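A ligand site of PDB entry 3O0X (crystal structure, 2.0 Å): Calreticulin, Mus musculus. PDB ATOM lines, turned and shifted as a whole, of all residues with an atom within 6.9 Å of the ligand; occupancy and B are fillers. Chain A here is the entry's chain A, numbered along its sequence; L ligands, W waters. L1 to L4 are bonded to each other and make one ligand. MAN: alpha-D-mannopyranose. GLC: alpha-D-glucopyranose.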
ATOM      1  N   PHE A  60      13.946 -10.752   3.344  1.00  0.00           N
ATOM      2  CA  PHE A  60      13.242 -10.552   4.600  1.00  0.00           C
ATOM      3  C   PHE A  60      13.217  -9.064   4.983  1.00  0.00           C
ATOM      4  O   PHE A  60      14.153  -8.329   4.693  1.00  0.00           O
ATOM      5  CB  PHE A  60      13.881 -11.377   5.723  1.00  0.00           C
ATOM      6  CG  PHE A  60      13.669 -12.867   5.573  1.00  0.00           C
ATOM      7  CD1 PHE A  60      12.500 -13.461   6.029  1.00  0.00           C
ATOM      8  CD2 PHE A  60      14.652 -13.666   4.995  1.00  0.00           C
ATOM      9  CE1 PHE A  60      12.289 -14.836   5.895  1.00  0.00           C
ATOM     10  CE2 PHE A  60      14.462 -15.053   4.867  1.00  0.00           C
ATOM     11  CZ  PHE A  60      13.272 -15.635   5.317  1.00  0.00           C
ATOM     12  N   TYR A  61      12.120  -8.644   5.610  1.00  0.00           N
ATOM     13  CA  TYR A  61      11.931  -7.271   6.065  1.00  0.00           C
ATOM     14  C   TYR A  61      11.699  -7.296   7.575  1.00  0.00           C
ATOM     15  O   TYR A  61      11.094  -8.235   8.086  1.00  0.00           O
ATOM     16  CB  TYR A  61      10.747  -6.604   5.344  1.00  0.00           C
ATOM     17  CG  TYR A  61      11.067  -6.332   3.898  1.00  0.00           C
ATOM     18  CD1 TYR A  61      10.941  -7.340   2.941  1.00  0.00           C
ATOM     19  CD2 TYR A  61      11.519  -5.076   3.490  1.00  0.00           C
ATOM     20  CE1 TYR A  61      11.269  -7.094   1.606  1.00  0.00           C
ATOM     21  CE2 TYR A  61      11.835  -4.830   2.162  1.00  0.00           C
ATOM     22  CZ  TYR A  61      11.727  -5.846   1.233  1.00  0.00           C
ATOM     23  OH  TYR A  61      12.039  -5.612  -0.088  1.00  0.00           O
ATOM     24  N   CYS A  91       4.355 -14.229  -3.926  1.00  0.00           N
ATOM     25  CA  CYS A  91       4.562 -14.748  -2.584  1.00  0.00           C
ATOM     26  C   CYS A  91       5.102 -13.641  -1.694  1.00  0.00           C
ATOM     27  O   CYS A  91       6.135 -13.017  -2.004  1.00  0.00           O
ATOM     28  CB  CYS A  91       5.520 -15.944  -2.615  1.00  0.00           C
ATOM     29  SG  CYS A  91       6.177 -16.413  -0.991  1.00  0.00           S
ATOM     30  N   GLY A  92       4.422 -13.389  -0.578  1.00  0.00           N
ATOM     31  CA  GLY A  92       4.853 -12.320   0.309  1.00  0.00           C
ATOM     32  C   GLY A  92       3.848 -11.972   1.394  1.00  0.00           C
ATOM     33  O   GLY A  92       2.639 -12.016   1.169  1.00  0.00           O
ATOM     34  N   GLY A  93       4.375 -11.640   2.568  1.00  0.00           N
ATOM     35  CA  GLY A  93       3.529 -11.319   3.699  1.00  0.00           C
ATOM     36  C   GLY A  93       2.992  -9.918   3.636  1.00  0.00           C
ATOM     37  O   GLY A  93       3.554  -9.072   2.957  1.00  0.00           O
ATOM     38  N   GLY A  94       1.866  -9.676   4.315  1.00  0.00           N
ATOM     39  CA  GLY A  94       1.339  -8.320   4.468  1.00  0.00           C
ATOM     40  C   GLY A  94       0.684  -8.185   5.830  1.00  0.00           C
ATOM     41  O   GLY A  94      -0.327  -7.514   5.959  1.00  0.00           O
ATOM     42  N   TYR A  95       1.242  -8.853   6.834  1.00  0.00           N
ATOM     43  CA  TYR A  95       0.697  -8.830   8.195  1.00  0.00           C
ATOM     44  C   TYR A  95       1.594  -8.059   9.161  1.00  0.00           C
ATOM     45  O   TYR A  95       2.750  -7.796   8.866  1.00  0.00           O
ATOM     46  CB  TYR A  95       0.487 -10.273   8.717  1.00  0.00           C
ATOM     47  CG  TYR A  95       1.651 -11.177   8.455  1.00  0.00           C
ATOM     48  CD1 TYR A  95       1.677 -12.005   7.326  1.00  0.00           C
ATOM     49  CD2 TYR A  95       2.759 -11.197   9.320  1.00  0.00           C
ATOM     50  CE1 TYR A  95       2.757 -12.832   7.074  1.00  0.00           C
ATOM     51  CE2 TYR A  95       3.843 -12.030   9.075  1.00  0.00           C
ATOM     52  CZ  TYR A  95       3.828 -12.854   7.948  1.00  0.00           C
ATOM     53  OH  TYR A  95       4.873 -13.684   7.656  1.00  0.00           O
ATOM     54  N   LYS A  97       2.816  -7.633  13.477  1.00  0.00           N
ATOM     55  CA  LYS A  97       2.922  -8.285  14.764  1.00  0.00           C
ATOM     56  C   LYS A  97       2.895  -7.241  15.867  1.00  0.00           C
ATOM     57  O   LYS A  97       3.482  -6.163  15.722  1.00  0.00           O
ATOM     58  CB  LYS A  97       4.216  -9.097  14.856  1.00  0.00           C
ATOM     59  CG  LYS A  97       4.212 -10.431  14.124  1.00  0.00           C
ATOM     60  CD  LYS A  97       5.618 -11.026  14.077  1.00  0.00           C
ATOM     61  CE  LYS A  97       5.614 -12.477  13.578  1.00  0.00           C
ATOM     62  NZ  LYS A  97       7.006 -13.053  13.512  1.00  0.00           N
ATOM     63  N   HIS A 109      13.301 -10.082  14.781  1.00  0.00           N
ATOM     64  CA  HIS A 109      13.302 -11.009  13.653  1.00  0.00           C
ATOM     65  C   HIS A 109      12.103 -11.944  13.708  1.00  0.00           C
ATOM     66  O   HIS A 109      11.216 -11.801  14.572  1.00  0.00           O
ATOM     67  CB  HIS A 109      14.631 -11.784  13.583  1.00  0.00           C
ATOM     68  CG  HIS A 109      14.928 -12.588  14.819  1.00  0.00           C
ATOM     69  ND1 HIS A 109      15.493 -12.026  15.952  1.00  0.00           N
ATOM     70  CD2 HIS A 109      14.741 -13.896  15.094  1.00  0.00           C
ATOM     71  CE1 HIS A 109      15.638 -12.961  16.874  1.00  0.00           C
ATOM     72  NE2 HIS A 109      15.186 -14.102  16.374  1.00  0.00           N
ATOM     73  N   GLY A 110      12.059 -12.912  12.793  1.00  0.00           N
ATOM     74  CA  GLY A 110      10.942 -13.837  12.688  1.00  0.00           C
ATOM     75  C   GLY A 110      10.584 -14.623  13.935  1.00  0.00           C
ATOM     76  O   GLY A 110       9.421 -14.944  14.162  1.00  0.00           O
ATOM     77  N   ASP A 111      11.585 -14.949  14.755  1.00  0.00           N
ATOM     78  CA  ASP A 111      11.328 -15.751  15.960  1.00  0.00           C
ATOM     79  C   ASP A 111      11.284 -14.948  17.251  1.00  0.00           C
ATOM     80  O   ASP A 111      11.203 -15.520  18.328  1.00  0.00           O
ATOM     81  CB  ASP A 111      12.321 -16.910  16.079  1.00  0.00           C
ATOM     82  CG  ASP A 111      12.305 -17.832  14.874  1.00  0.00           C
ATOM     83  OD1 ASP A 111      11.214 -17.999  14.256  1.00  0.00           O
ATOM     84  OD2 ASP A 111      13.371 -18.375  14.545  1.00  0.00           O
ATOM     85  N   SER A 112      11.339 -13.616  17.128  1.00  0.00           N
ATOM     86  CA  SER A 112      11.129 -12.744  18.278  1.00  0.00           C
ATOM     87  C   SER A 112       9.724 -13.009  18.814  1.00  0.00           C
ATOM     88  O   SER A 112       8.773 -13.147  18.027  1.00  0.00           O
ATOM     89  CB  SER A 112      11.275 -11.282  17.868  1.00  0.00           C
ATOM     90  OG  SER A 112      12.587 -11.025  17.407  1.00  0.00           O
ATOM     91  N   TYR A 114       6.118 -12.576  20.126  1.00  0.00           N
ATOM     92  CA  TYR A 114       5.081 -11.557  19.935  1.00  0.00           C
ATOM     93  C   TYR A 114       3.806 -11.929  20.697  1.00  0.00           C
ATOM     94  O   TYR A 114       3.651 -13.081  21.145  1.00  0.00           O
ATOM     95  CB  TYR A 114       4.779 -11.359  18.433  1.00  0.00           C
ATOM     96  CG  TYR A 114       4.356 -12.638  17.715  1.00  0.00           C
ATOM     97  CD1 TYR A 114       5.292 -13.457  17.074  1.00  0.00           C
ATOM     98  CD2 TYR A 114       3.018 -13.025  17.677  1.00  0.00           C
ATOM     99  CE1 TYR A 114       4.914 -14.613  16.426  1.00  0.00           C
ATOM    100  CE2 TYR A 114       2.629 -14.199  17.036  1.00  0.00           C
ATOM    101  CZ  TYR A 114       3.588 -14.984  16.410  1.00  0.00           C
ATOM    102  OH  TYR A 114       3.207 -16.135  15.785  1.00  0.00           O
ATOM    103  N   MET A 117      -0.297 -11.702  15.977  1.00  0.00           N
ATOM    104  CA  MET A 117       0.069 -11.491  14.580  1.00  0.00           C
ATOM    105  C   MET A 117      -1.221 -11.462  13.747  1.00  0.00           C
ATOM    106  O   MET A 117      -2.064 -12.320  13.929  1.00  0.00           O
ATOM    107  CB  MET A 117       0.999 -12.599  14.088  1.00  0.00           C
ATOM    108  CG  MET A 117       1.331 -12.541  12.568  1.00  0.00           C
ATOM    109  SD  MET A 117       2.607 -13.924  12.015  1.00  0.00           S
ATOM    110  CE  MET A 117       1.675 -14.599  10.462  1.00  0.00           C
ATOM    111  N   PRO A 120      -2.970 -10.317   5.978  1.00  0.00           N
ATOM    112  CA  PRO A 120      -2.941 -11.200   4.809  1.00  0.00           C
ATOM    113  C   PRO A 120      -1.557 -11.798   4.571  1.00  0.00           C
ATOM    114  O   PRO A 120      -0.544 -11.115   4.771  1.00  0.00           O
ATOM    115  CB  PRO A 120      -3.344 -10.272   3.659  1.00  0.00           C
ATOM    116  CG  PRO A 120      -2.951  -8.871   4.125  1.00  0.00           C
ATOM    117  CD  PRO A 120      -3.135  -8.893   5.619  1.00  0.00           C
ATOM    118  N   ASP A 121      -1.528 -13.077   4.197  1.00  0.00           N
ATOM    119  CA  ASP A 121      -0.319 -13.776   3.770  1.00  0.00           C
ATOM    120  C   ASP A 121      -0.654 -14.443   2.432  1.00  0.00           C
ATOM    121  O   ASP A 121      -1.726 -15.033   2.271  1.00  0.00           O
ATOM    122  CB  ASP A 121       0.095 -14.851   4.802  1.00  0.00           C
ATOM    123  CG  ASP A 121       1.518 -15.385   4.581  1.00  0.00           C
ATOM    124  OD1 ASP A 121       2.322 -14.774   3.828  1.00  0.00           O
ATOM    125  OD2 ASP A 121       1.838 -16.452   5.171  1.00  0.00           O
ATOM    126  N   ILE A 122       0.236 -14.276   1.456  1.00  0.00           N
ATOM    127  CA  ILE A 122       0.078 -14.863   0.128  1.00  0.00           C
ATOM    128  C   ILE A 122       1.366 -15.633  -0.174  1.00  0.00           C
ATOM    129  O   ILE A 122       2.460 -15.105   0.052  1.00  0.00           O
ATOM    130  CB  ILE A 122      -0.189 -13.750  -0.959  1.00  0.00           C
ATOM    131  CG1 ILE A 122      -1.537 -13.050  -0.680  1.00  0.00           C
ATOM    132  CG2 ILE A 122      -0.084 -14.302  -2.399  1.00  0.00           C
ATOM    133  CD1 ILE A 122      -1.863 -11.876  -1.617  1.00  0.00           C
ATOM    134  N   CYS A 123       1.232 -16.877  -0.615  1.00  0.00           N
ATOM    135  CA  CYS A 123       2.398 -17.652  -1.052  1.00  0.00           C
ATOM    136  C   CYS A 123       1.988 -18.668  -2.106  1.00  0.00           C
ATOM    137  O   CYS A 123       1.620 -19.788  -1.786  1.00  0.00           O
ATOM    138  CB  CYS A 123       3.067 -18.336   0.123  1.00  0.00           C
ATOM    139  SG  CYS A 123       4.708 -18.943  -0.266  1.00  0.00           S
ATOM    140  N   THR A 127      -1.535 -20.592  -0.693  1.00  0.00           N
ATOM    141  CA  THR A 127      -1.625 -19.780   0.531  1.00  0.00           C
ATOM    142  C   THR A 127      -2.193 -18.419   0.154  1.00  0.00           C
ATOM    143  O   THR A 127      -1.553 -17.659  -0.571  1.00  0.00           O
ATOM    144  CB  THR A 127      -0.246 -19.628   1.238  1.00  0.00           C
ATOM    145  OG1 THR A 127       0.249 -20.907   1.653  1.00  0.00           O
ATOM    146  CG2 THR A 127      -0.354 -18.725   2.484  1.00  0.00           C
ATOM    147  N   HIS A 131      -4.055 -14.262   8.528  1.00  0.00           N
ATOM    148  CA  HIS A 131      -3.634 -14.816   9.805  1.00  0.00           C
ATOM    149  C   HIS A 131      -4.216 -14.049  10.968  1.00  0.00           C
ATOM    150  O   HIS A 131      -4.320 -12.821  10.924  1.00  0.00           O
ATOM    151  CB  HIS A 131      -2.106 -14.828   9.915  1.00  0.00           C
ATOM    152  CG  HIS A 131      -1.481 -16.014   9.258  1.00  0.00           C
ATOM    153  ND1 HIS A 131      -1.613 -17.296   9.751  1.00  0.00           N
ATOM    154  CD2 HIS A 131      -0.725 -16.118   8.134  1.00  0.00           C
ATOM    155  CE1 HIS A 131      -0.963 -18.136   8.955  1.00  0.00           C
ATOM    156  NE2 HIS A 131      -0.411 -17.441   7.981  1.00  0.00           N
ATOM    157  N   ILE A 133      -3.260 -14.779  14.900  1.00  0.00           N
ATOM    158  CA  ILE A 133      -2.504 -15.641  15.808  1.00  0.00           C
ATOM    159  C   ILE A 133      -2.410 -15.004  17.200  1.00  0.00           C
ATOM    160  O   ILE A 133      -1.978 -13.853  17.332  1.00  0.00           O
ATOM    161  CB  ILE A 133      -1.063 -15.903  15.286  1.00  0.00           C
ATOM    162  CG1 ILE A 133      -1.089 -16.447  13.841  1.00  0.00           C
ATOM    163  CG2 ILE A 133      -0.299 -16.843  16.223  1.00  0.00           C
ATOM    164  CD1 ILE A 133       0.264 -16.824  13.273  1.00  0.00           C
ATOM    165  N   ASN A 140       2.145 -20.027  20.063  1.00  0.00           N
ATOM    166  CA  ASN A 140       1.450 -19.212  19.049  1.00  0.00           C
ATOM    167  C   ASN A 140       0.311 -20.010  18.408  1.00  0.00           C
ATOM    168  O   ASN A 140       0.565 -20.989  17.688  1.00  0.00           O
ATOM    169  CB  ASN A 140       2.425 -18.693  17.974  1.00  0.00           C
ATOM    170  CG  ASN A 140       3.613 -17.959  18.565  1.00  0.00           C
ATOM    171  OD1 ASN A 140       3.478 -17.153  19.485  1.00  0.00           O
ATOM    172  ND2 ASN A 140       4.797 -18.245  18.035  1.00  0.00           N
ATOM    173  N   LEU A 142      -2.822 -20.449  15.884  1.00  0.00           N
ATOM    174  CA  LEU A 142      -3.402 -19.966  14.639  1.00  0.00           C
ATOM    175  C   LEU A 142      -4.904 -20.171  14.646  1.00  0.00           C
ATOM    176  O   LEU A 142      -5.389 -21.202  15.122  1.00  0.00           O
ATOM    177  CB  LEU A 142      -2.806 -20.718  13.448  1.00  0.00           C
ATOM    178  CG  LEU A 142      -1.450 -20.255  12.886  1.00  0.00           C
ATOM    179  CD1 LEU A 142      -0.341 -20.410  13.919  1.00  0.00           C
ATOM    180  CD2 LEU A 142      -1.114 -21.029  11.630  1.00  0.00           C
ATOM    181  N   ASP A 214       7.397  -7.947  10.031  1.00  0.00           N
ATOM    182  CA  ASP A 214       8.342  -9.042   9.823  1.00  0.00           C
ATOM    183  C   ASP A 214       7.845  -9.859   8.647  1.00  0.00           C
ATOM    184  O   ASP A 214       6.869 -10.608   8.781  1.00  0.00           O
ATOM    185  CB  ASP A 214       8.423  -9.925  11.095  1.00  0.00           C
ATOM    186  CG  ASP A 214       8.782 -11.390  10.786  1.00  0.00           C
ATOM    187  OD1 ASP A 214       9.828 -11.643  10.139  1.00  0.00           O
ATOM    188  OD2 ASP A 214       8.011 -12.293  11.203  1.00  0.00           O
ATOM    189  N   LEU A 215       8.497  -9.710   7.498  1.00  0.00           N
ATOM    190  CA  LEU A 215       7.965 -10.232   6.240  1.00  0.00           C
ATOM    191  C   LEU A 215       9.035 -10.898   5.397  1.00  0.00           C
ATOM    192  O   LEU A 215      10.209 -10.542   5.477  1.00  0.00           O
ATOM    193  CB  LEU A 215       7.338  -9.093   5.409  1.00  0.00           C
ATOM    194  CG  LEU A 215       6.420  -8.066   6.064  1.00  0.00           C
ATOM    195  CD1 LEU A 215       6.146  -6.911   5.087  1.00  0.00           C
ATOM    196  CD2 LEU A 215       5.136  -8.723   6.529  1.00  0.00           C
ATOM    197  N   TRP A 216       8.619 -11.888   4.608  1.00  0.00           N
ATOM    198  CA  TRP A 216       9.375 -12.372   3.463  1.00  0.00           C
ATOM    199  C   TRP A 216       8.582 -11.989   2.216  1.00  0.00           C
ATOM    200  O   TRP A 216       7.363 -12.103   2.213  1.00  0.00           O
ATOM    201  CB  TRP A 216       9.545 -13.901   3.530  1.00  0.00           C
ATOM    202  CG  TRP A 216      10.027 -14.488   2.236  1.00  0.00           C
ATOM    203  CD1 TRP A 216       9.272 -15.147   1.307  1.00  0.00           C
ATOM    204  CD2 TRP A 216      11.367 -14.433   1.702  1.00  0.00           C
ATOM    205  NE1 TRP A 216      10.057 -15.503   0.234  1.00  0.00           N
ATOM    206  CE2 TRP A 216      11.342 -15.079   0.455  1.00  0.00           C
ATOM    207  CE3 TRP A 216      12.568 -13.898   2.171  1.00  0.00           C
ATOM    208  CZ2 TRP A 216      12.482 -15.225  -0.346  1.00  0.00           C
ATOM    209  CZ3 TRP A 216      13.720 -14.043   1.377  1.00  0.00           C
ATOM    210  CH2 TRP A 216      13.668 -14.702   0.137  1.00  0.00           C
ATOM    211  N   GLN A 217       9.257 -11.522   1.168  1.00  0.00           N
ATOM    212  CA  GLN A 217       8.616 -11.258  -0.118  1.00  0.00           C
ATOM    213  C   GLN A 217       9.482 -11.703  -1.273  1.00  0.00           C
ATOM    214  O   GLN A 217      10.701 -11.522  -1.237  1.00  0.00           O
ATOM    215  CB  GLN A 217       8.287  -9.766  -0.292  1.00  0.00           C
ATOM    216  CG  GLN A 217       7.312  -9.192   0.737  1.00  0.00           C
ATOM    217  CD  GLN A 217       6.413  -8.124   0.180  1.00  0.00           C
ATOM    218  OE1 GLN A 217       6.834  -7.289  -0.627  1.00  0.00           O
ATOM    219  NE2 GLN A 217       5.156  -8.139   0.613  1.00  0.00           N
ATOM    220  N   VAL A 218       8.851 -12.311  -2.291  1.00  0.00           N
ATOM    221  CA  VAL A 218       9.534 -12.615  -3.554  1.00  0.00           C
ATOM    222  C   VAL A 218       9.481 -11.388  -4.467  1.00  0.00           C
ATOM    223  O   VAL A 218      10.434 -10.626  -4.493  1.00  0.00           O
ATOM    224  CB  VAL A 218       9.026 -13.931  -4.213  1.00  0.00           C
ATOM    225  CG1 VAL A 218       9.903 -14.326  -5.408  1.00  0.00           C
ATOM    226  CG2 VAL A 218       9.045 -15.064  -3.184  1.00  0.00           C
HETATM  227  C1  MAN L   1       8.381 -19.315   1.116  1.00  0.00           C
HETATM  228  C2  MAN L   1       8.883 -18.933   2.465  1.00  0.00           C
HETATM  229  C3  MAN L   1      10.363 -18.982   2.654  1.00  0.00           C
HETATM  230  C4  MAN L   1      10.558 -20.495   2.671  1.00  0.00           C
HETATM  231  C5  MAN L   1      10.051 -21.051   1.330  1.00  0.00           C
HETATM  232  C6  MAN L   1      10.266 -22.557   1.198  1.00  0.00           C
HETATM  233  O1  MAN L   1       9.102 -18.644   0.074  1.00  0.00           O
HETATM  234  O2  MAN L   1       7.895 -18.790   3.513  1.00  0.00           O
HETATM  235  O3  MAN L   1      10.819 -18.407   3.878  1.00  0.00           O
HETATM  236  O4  MAN L   1      11.932 -20.832   2.880  1.00  0.00           O
HETATM  237  O5  MAN L   1       8.667 -20.716   1.079  1.00  0.00           O
HETATM  238  O6  MAN L   1       9.127 -23.273   1.671  1.00  0.00           O
HETATM  239  C1  MAN L   2       7.860 -17.652   4.367  1.00  0.00           C
HETATM  240  C2  MAN L   2       7.056 -18.181   5.560  1.00  0.00           C
HETATM  241  C3  MAN L   2       5.622 -18.508   5.148  1.00  0.00           C
HETATM  242  C4  MAN L   2       5.011 -17.323   4.413  1.00  0.00           C
HETATM  243  C5  MAN L   2       5.889 -16.892   3.230  1.00  0.00           C
HETATM  244  C6  MAN L   2       5.295 -15.680   2.524  1.00  0.00           C
HETATM  245  O2  MAN L   2       7.027 -17.232   6.620  1.00  0.00           O
HETATM  246  O3  MAN L   2       4.819 -18.789   6.295  1.00  0.00           O
HETATM  247  O4  MAN L   2       3.703 -17.684   3.970  1.00  0.00           O
HETATM  248  O5  MAN L   2       7.200 -16.551   3.713  1.00  0.00           O
HETATM  249  O6  MAN L   2       4.905 -14.720   3.514  1.00  0.00           O
HETATM  250  C1  MAN L   3       8.144 -17.297   7.481  1.00  0.00           C
HETATM  251  C2  MAN L   3       7.642 -17.596   8.894  1.00  0.00           C
HETATM  252  C3  MAN L   3       6.796 -16.448   9.440  1.00  0.00           C
HETATM  253  C4  MAN L   3       7.560 -15.123   9.326  1.00  0.00           C
HETATM  254  C5  MAN L   3       8.055 -14.899   7.894  1.00  0.00           C
HETATM  255  C6  MAN L   3       8.936 -13.662   7.766  1.00  0.00           C
HETATM  256  O2  MAN L   3       8.792 -17.804   9.736  1.00  0.00           O
HETATM  257  O3  MAN L   3       6.513 -16.719  10.814  1.00  0.00           O
HETATM  258  O4  MAN L   3       6.734 -14.035   9.753  1.00  0.00           O
HETATM  259  O5  MAN L   3       8.811 -16.027   7.432  1.00  0.00           O
HETATM  260  O6  MAN L   3      10.079 -13.743   8.625  1.00  0.00           O
HETATM  261  C1  GLC L   4       5.287 -16.197  11.350  1.00  0.00           C
HETATM  262  C2  GLC L   4       5.277 -16.315  12.876  1.00  0.00           C
HETATM  263  C3  GLC L   4       5.075 -17.769  13.318  1.00  0.00           C
HETATM  264  C4  GLC L   4       3.825 -18.372  12.662  1.00  0.00           C
HETATM  265  C5  GLC L   4       3.891 -18.195  11.137  1.00  0.00           C
HETATM  266  C6  GLC L   4       2.603 -18.598  10.421  1.00  0.00           C
HETATM  267  O2  GLC L   4       6.496 -15.771  13.387  1.00  0.00           O
HETATM  268  O3  GLC L   4       4.937 -17.819  14.735  1.00  0.00           O
HETATM  269  O4  GLC L   4       3.709 -19.774  12.982  1.00  0.00           O
HETATM  270  O5  GLC L   4       4.130 -16.823  10.794  1.00  0.00           O
HETATM  271  O6  GLC L   4       2.833 -18.504   8.994  1.00  0.00           O
HETATM  272  O   HOH W   1       5.897 -21.168   7.688  1.00  0.00           O
HETATM  273  O   HOH W   2      11.124 -16.245   9.563  1.00  0.00           O
HETATM  274  O   HOH W   3       4.596 -20.759  15.763  1.00  0.00           O
HETATM  275  O   HOH W   4       3.640 -16.293   7.552  1.00  0.00           O
HETATM  276  O   HOH W   5       5.730 -21.361  11.782  1.00  0.00           O
HETATM  277  O   HOH W   6       6.079 -13.041   5.291  1.00  0.00           O
HETATM  278  O   HOH W   7       8.599 -17.515  12.759  1.00  0.00           O
HETATM  279  O   HOH W   8       7.508 -17.268  16.178  1.00  0.00           O
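O4 of MAN L2 is in hydrogen-bond range of OD2 of Asp 121 (2.5 Å).
The side-chain carboxylate (OD1) of Asp 214 lies within hydrogen-bond range of an oxygen (O6) of MAN L3.
The side-chain hydroxyl of Tyr 114 is in hydrogen-bond range of an oxygen (O3) of GLC L4, at 2.6 Å.
O2 of GLC L4 sits at hydrogen-bond distance from NZ of Lys 97, 2.8 Å away.
OH of Tyr 95 sits at hydrogen-bond distance from O4 of MAN L3.
The backbone carbonyl oxygen (O) of Gly 110 lies within hydrogen-bond range of an oxygen (O2) of GLC L4 (3.1 Å).
The backbone NH (N) of Gly 93 sits at hydrogen-bond distance from an oxygen (O6) of MAN L2 (3.3 Å).
O1 of MAN L1 sits at hydrogen-bond distance from NE1 of Trp 216, 3.3 Å away.
The side-chain amide nitrogen (ND2) of Asn 140 is in hydrogen-bond range of an oxygen (O3) of GLC L4, at 3.3 Å.
The side-chain carboxylate of Asp 214 lies within salt-bridge range of the side-chain amino group of Lys 97 (2.6 Å).
The side-chain hydroxyl (OH) of Tyr 114 lies close to the side-chain amide nitrogen (ND2) of Asn 140 (3.5 Å).
The backbone carbonyl oxygen (O) of Gly 110 is in hydrogen-bond range of the side-chain amino group (NZ) of Lys 97 (3.1 Å).
The backbone NH (N) of Gly 93 lies within hydrogen-bond range of the backbone carbonyl oxygen (O) of Trp 216, 3.0 Å away.
O of Met 117 is in hydrogen-bond range of N of Ile 133, 2.9 Å away.
The backbone NH (N) of Gly 92 sits at hydrogen-bond distance from the backbone carbonyl oxygen (O) of Ile 122 (2.7 Å).
O of Leu 215 lies within hydrogen-bond range of N of Tyr 61, at 2.7 Å.
The backbone NH (N) of Val 218 is in hydrogen-bond range of the backbone carbonyl oxygen (O) of Cys 91 (2.8 Å).
An oxygen (O5) of GLC L4 lies close to the side-chain sulfur (SD) of Met 117 (3.5 Å).
CD1 of Phe 60 touches O6 of MAN L3, at 3.6 Å.
SG of Cys 91 touches C6 of MAN L2 (3.7 Å).
Gly 92 touches the ligand.
Ile 122 touches the ligand.
Cys 123 touches the ligand.
NE2 of His 131 touches O6 of GLC L4, at 3.6 Å.
CD1 of Ile 133 touches C4 of GLC L4 (3.9 Å).
C of Leu 215 touches C6 of MAN L3, 3.6 Å away.
18 residues have an atom within 4 Å of the ligand: Phe 60, Cys 91, Gly 92, Gly 93, Tyr 95, Lys 97, Gly 110, Tyr 114, Met 117, Asp 121, Ile 122, Cys 123, His 131, Ile 133, Asn 140, Asp 214, Leu 215 and Trp 216.
Along chain A the residues within 4 Å of the ligand span positions 60 to 216.
Water W6 lies within hydrogen-bond range of O6 of MAN L2 (2.7 Å), OH of Tyr 95 (2.7 Å) and N of Trp 216 (2.9 Å).
Water W4 lies within hydrogen-bond range of an oxygen (O6) of GLC L4 (2.8 Å), the side-chain hydroxyl (OH) of Tyr 95 (2.9 Å) and the side-chain carboxylate (OD2) of Asp 121 (3.0 Å).
Water W7 lies within hydrogen-bond range of O2 of GLC L4 (2.8 Å), O of Gly 110 (3.0 Å) and OD1 of Asp 111 (3.1 Å).
Water W8 lies within hydrogen-bond range of O3 of GLC L4 and ND2 of Asn 140.
Water W3 bridges an oxygen (O4) of GLC L4 (3.1 Å) and the side-chain amide nitrogen of Asn 140 (3.4 Å).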
